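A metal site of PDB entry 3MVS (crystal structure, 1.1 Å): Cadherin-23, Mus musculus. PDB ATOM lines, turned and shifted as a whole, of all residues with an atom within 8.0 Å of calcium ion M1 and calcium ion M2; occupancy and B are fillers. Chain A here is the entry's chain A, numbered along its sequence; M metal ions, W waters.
The backbone NH (N) of Glu 120 sits at hydrogen-bond distance from the backbone carbonyl oxygen (O) of Thr 204, 3.0 Å away. The backbone NH (N) of Tyr 172 sits close to the side-chain carboxylate (OE1) of Glu 120, at 2.9 Å.
Of the 16 residues printed, 5 come within 4 Å of calcium ion M1. The nearest printed residue that does not touch calcium ion M1 is Gln 207 (4.6 Å).
Of the 16 residues printed, 4 come within 4 Å of calcium ion M2.
Calcium ion M1 is bound by OD1 of Asp 205 (2.3 Å), OD1 of Asp 208 (2.4 Å), O of Met 206 (2.4 Å), OE2 of Glu 173 (2.4 Å), OE2 of Glu 120 (2.4 Å), water W1 (2.4 Å) and OE1 of Glu 173 (2.9 Å).
Calcium ion M2 is bound by the side-chain carboxylate (OE1) of Glu 173 (2.3 Å), the side-chain carboxylate (OD1) of Asp 171 (2.3 Å), water W2 (2.3 Å), water W3 (2.4 Å), the side-chain carboxylate (OE1) of Glu 120 (2.4 Å) and the side-chain carboxylate (OD2) of Asp 208 (2.4 Å).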
ATOM      1  N   GLU A 120      27.128   4.733   3.877  1.00  0.00           N
ATOM      2  CA  GLU A 120      28.361   4.756   4.669  1.00  0.00           C
ATOM      3  C   GLU A 120      28.869   3.350   5.001  1.00  0.00           C
ATOM      4  O   GLU A 120      30.050   3.205   5.319  1.00  0.00           O
ATOM      5  CB  GLU A 120      28.259   5.585   5.957  1.00  0.00           C
ATOM      6  CG  GLU A 120      27.236   5.049   6.963  1.00  0.00           C
ATOM      7  CD  GLU A 120      27.294   5.776   8.290  1.00  0.00           C
ATOM      8  OE1 GLU A 120      28.414   6.073   8.779  1.00  0.00           O
ATOM      9  OE2 GLU A 120      26.208   6.020   8.860  1.00  0.00           O
ATOM     10  N   ASN A 121      28.009   2.321   4.912  1.00  0.00           N
ATOM     11  CA  ASN A 121      28.472   0.946   5.147  1.00  0.00           C
ATOM     12  C   ASN A 121      28.785   0.171   3.856  1.00  0.00           C
ATOM     13  O   ASN A 121      28.863  -1.051   3.865  1.00  0.00           O
ATOM     14  CB  ASN A 121      27.509   0.166   6.047  1.00  0.00           C
ATOM     15  CG  ASN A 121      26.161  -0.075   5.391  1.00  0.00           C
ATOM     16  OD1 ASN A 121      25.833   0.521   4.373  1.00  0.00           O
ATOM     17  ND2 ASN A 121      25.390  -0.976   5.987  1.00  0.00           N
ATOM     18  N   GLU A 169      36.897   2.164   4.921  1.00  0.00           N
ATOM     19  CA  GLU A 169      35.574   2.281   5.483  1.00  0.00           C
ATOM     20  C   GLU A 169      35.130   3.744   5.587  1.00  0.00           C
ATOM     21  O   GLU A 169      35.881   4.622   6.048  1.00  0.00           O
ATOM     22  CB  GLU A 169      35.536   1.650   6.866  1.00  0.00           C
ATOM     23  CG  GLU A 169      34.168   1.772   7.512  1.00  0.00           C
ATOM     24  CD  GLU A 169      33.983   0.936   8.742  1.00  0.00           C
ATOM     25  OE1 GLU A 169      34.992   0.484   9.318  1.00  0.00           O
ATOM     26  OE2 GLU A 169      32.807   0.735   9.136  1.00  0.00           O
ATOM     27  N   LEU A 170      33.879   3.991   5.173  1.00  0.00           N
ATOM     28  CA  LEU A 170      33.301   5.336   5.204  1.00  0.00           C
ATOM     29  C   LEU A 170      32.591   5.583   6.526  1.00  0.00           C
ATOM     30  O   LEU A 170      32.334   4.647   7.266  1.00  0.00           O
ATOM     31  CB  LEU A 170      32.341   5.494   4.022  1.00  0.00           C
ATOM     32  CG  LEU A 170      32.977   5.238   2.657  1.00  0.00           C
ATOM     33  CD1 LEU A 170      31.944   4.835   1.583  1.00  0.00           C
ATOM     34  CD2 LEU A 170      33.797   6.457   2.223  1.00  0.00           C
ATOM     35  N   ASP A 171      32.325   6.834   6.830  1.00  0.00           N
ATOM     36  CA  ASP A 171      31.673   7.189   8.079  1.00  0.00           C
ATOM     37  C   ASP A 171      30.958   8.523   7.910  1.00  0.00           C
ATOM     38  O   ASP A 171      31.607   9.583   7.913  1.00  0.00           O
ATOM     39  CB  ASP A 171      32.700   7.250   9.230  1.00  0.00           C
ATOM     40  CG  ASP A 171      32.040   7.431  10.575  1.00  0.00           C
ATOM     41  OD1 ASP A 171      30.793   7.501  10.653  1.00  0.00           O
ATOM     42  OD2 ASP A 171      32.798   7.488  11.573  1.00  0.00           O
ATOM     43  N   TYR A 172      29.633   8.477   7.769  1.00  0.00           N
ATOM     44  CA  TYR A 172      28.830   9.649   7.564  1.00  0.00           C
ATOM     45  C   TYR A 172      29.052  10.664   8.688  1.00  0.00           C
ATOM     46  O   TYR A 172      29.023  11.873   8.463  1.00  0.00           O
ATOM     47  CB  TYR A 172      27.342   9.235   7.529  1.00  0.00           C
ATOM     48  CG  TYR A 172      26.441  10.403   7.359  1.00  0.00           C
ATOM     49  CD1 TYR A 172      26.065  10.823   6.077  1.00  0.00           C
ATOM     50  CD2 TYR A 172      25.940  11.098   8.465  1.00  0.00           C
ATOM     51  CE1 TYR A 172      25.218  11.931   5.908  1.00  0.00           C
ATOM     52  CE2 TYR A 172      25.111  12.199   8.311  1.00  0.00           C
ATOM     53  CZ  TYR A 172      24.757  12.609   7.025  1.00  0.00           C
ATOM     54  OH  TYR A 172      23.925  13.682   6.835  1.00  0.00           O
ATOM     55  N   GLU A 173      29.261  10.166   9.903  1.00  0.00           N
ATOM     56  CA  GLU A 173      29.452  11.007  11.077  1.00  0.00           C
ATOM     57  C   GLU A 173      30.746  11.846  11.003  1.00  0.00           C
ATOM     58  O   GLU A 173      30.922  12.788  11.770  1.00  0.00           O
ATOM     59  CB  GLU A 173      29.426  10.139  12.343  1.00  0.00           C
ATOM     60  CG  GLU A 173      28.010   9.738  12.825  1.00  0.00           C
ATOM     61  CD  GLU A 173      27.265   8.708  11.960  1.00  0.00           C
ATOM     62  OE1 GLU A 173      27.853   7.796  11.348  1.00  0.00           O
ATOM     63  OE2 GLU A 173      26.019   8.813  11.907  1.00  0.00           O
ATOM     64  N   VAL A 174      31.642  11.472  10.102  1.00  0.00           N
ATOM     65  CA  VAL A 174      32.858  12.253   9.850  1.00  0.00           C
ATOM     66  C   VAL A 174      32.696  13.075   8.569  1.00  0.00           C
ATOM     67  O   VAL A 174      32.913  14.281   8.566  1.00  0.00           O
ATOM     68  CB  VAL A 174      34.106  11.344   9.763  1.00  0.00           C
ATOM     69  CG1 VAL A 174      35.330  12.172   9.336  1.00  0.00           C
ATOM     70  CG2 VAL A 174      34.372  10.669  11.106  1.00  0.00           C
ATOM     71  N   ILE A 203      27.261  10.582   0.740  1.00  0.00           N
ATOM     72  CA  ILE A 203      27.211   9.466   1.688  1.00  0.00           C
ATOM     73  C   ILE A 203      25.836   9.429   2.354  1.00  0.00           C
ATOM     74  O   ILE A 203      25.394  10.425   2.924  1.00  0.00           O
ATOM     75  CB  ILE A 203      28.319   9.584   2.759  1.00  0.00           C
ATOM     76  CG1 ILE A 203      29.714   9.767   2.109  1.00  0.00           C
ATOM     77  CG2 ILE A 203      28.290   8.369   3.669  1.00  0.00           C
ATOM     78  CD1 ILE A 203      30.129   8.650   1.144  1.00  0.00           C
ATOM     79  N   THR A 204      25.166   8.279   2.262  1.00  0.00           N
ATOM     80  CA  THR A 204      23.922   8.013   2.998  1.00  0.00           C
ATOM     81  C   THR A 204      24.227   7.645   4.443  1.00  0.00           C
ATOM     82  O   THR A 204      25.045   6.752   4.719  1.00  0.00           O
ATOM     83  CB  THR A 204      23.192   6.896   2.309  1.00  0.00           C
ATOM     84  OG1 THR A 204      22.774   7.356   1.022  1.00  0.00           O
ATOM     85  CG2 THR A 204      21.931   6.433   3.081  1.00  0.00           C
ATOM     86  N   ASP A 205      23.614   8.364   5.369  1.00  0.00           N
ATOM     87  CA  ASP A 205      23.717   8.049   6.787  1.00  0.00           C
ATOM     88  C   ASP A 205      22.971   6.756   7.052  1.00  0.00           C
ATOM     89  O   ASP A 205      21.789   6.639   6.754  1.00  0.00           O
ATOM     90  CB  ASP A 205      23.098   9.198   7.574  1.00  0.00           C
ATOM     91  CG  ASP A 205      23.321   9.084   9.067  1.00  0.00           C
ATOM     92  OD1 ASP A 205      24.162   8.259   9.479  1.00  0.00           O
ATOM     93  OD2 ASP A 205      22.629   9.833   9.796  1.00  0.00           O
ATOM     94  N   MET A 206      23.657   5.762   7.593  1.00  0.00           N
ATOM     95  CA  MET A 206      23.033   4.522   8.015  1.00  0.00           C
ATOM     96  C   MET A 206      22.851   4.528   9.524  1.00  0.00           C
ATOM     97  O   MET A 206      23.566   5.232  10.240  1.00  0.00           O
ATOM     98  CB  MET A 206      23.878   3.324   7.579  1.00  0.00           C
ATOM     99  CG  MET A 206      24.122   3.251   6.085  1.00  0.00           C
ATOM    100  SD  MET A 206      22.640   3.117   5.062  1.00  0.00           S
ATOM    101  CE  MET A 206      22.183   1.448   5.465  1.00  0.00           C
ATOM    102  N   GLN A 207      21.879   3.765  10.004  1.00  0.00           N
ATOM    103  CA  GLN A 207      21.614   3.691  11.431  1.00  0.00           C
ATOM    104  C   GLN A 207      22.633   2.733  12.026  1.00  0.00           C
ATOM    105  O   GLN A 207      22.392   1.542  12.105  1.00  0.00           O
ATOM    106  CB  GLN A 207      20.159   3.272  11.671  1.00  0.00           C
ATOM    107  CG  GLN A 207      19.205   4.326  11.141  1.00  0.00           C
ATOM    108  CD  GLN A 207      17.817   4.103  11.645  1.00  0.00           C
ATOM    109  OE1 GLN A 207      17.581   4.191  12.858  1.00  0.00           O
ATOM    110  NE2 GLN A 207      16.880   3.817  10.742  1.00  0.00           N
ATOM    111  N   ASP A 208      23.794   3.261  12.394  1.00  0.00           N
ATOM    112  CA  ASP A 208      24.934   2.425  12.728  1.00  0.00           C
ATOM    113  C   ASP A 208      25.548   2.735  14.075  1.00  0.00           C
ATOM    114  O   ASP A 208      26.760   2.577  14.277  1.00  0.00           O
ATOM    115  CB  ASP A 208      26.009   2.511  11.614  1.00  0.00           C
ATOM    116  CG  ASP A 208      26.681   3.877  11.518  1.00  0.00           C
ATOM    117  OD1 ASP A 208      26.118   4.917  11.954  1.00  0.00           O
ATOM    118  OD2 ASP A 208      27.809   3.907  10.984  1.00  0.00           O
ATOM    119  N   MET A 209      24.721   3.190  15.023  1.00  0.00           N
ATOM    120  CA  MET A 209      25.237   3.456  16.361  1.00  0.00           C
ATOM    121  C   MET A 209      25.754   2.146  16.965  1.00  0.00           C
ATOM    122  O   MET A 209      25.088   1.118  16.870  1.00  0.00           O
ATOM    123  CB  MET A 209      24.159   4.087  17.239  1.00  0.00           C
ATOM    124  CG  MET A 209      24.718   4.873  18.418  1.00  0.00           C
ATOM    125  SD  MET A 209      23.495   5.884  19.267  1.00  0.00           S
ATOM    126  CE  MET A 209      22.760   6.808  17.922  1.00  0.00           C
ATOM    127  N   ASP A 210      26.966   2.172  17.524  1.00  0.00           N
ATOM    128  CA  ASP A 210      27.519   1.015  18.229  1.00  0.00           C
ATOM    129  C   ASP A 210      26.914   0.902  19.632  1.00  0.00           C
ATOM    130  O   ASP A 210      26.406   1.891  20.171  1.00  0.00           O
HETATM  131 CA    CA M   1      25.215   6.813  10.893  1.00  0.00          CA
HETATM  132 CA    CA M   2      29.126   5.894  11.038  1.00  0.00          CA
HETATM  133  O   HOH W   1      23.480   6.987  12.580  1.00  0.00           O
HETATM  134  O   HOH W   2      29.295   5.949  13.379  1.00  0.00           O
HETATM  135  O   HOH W   3      30.765   4.468  10.080  1.00  0.00           O
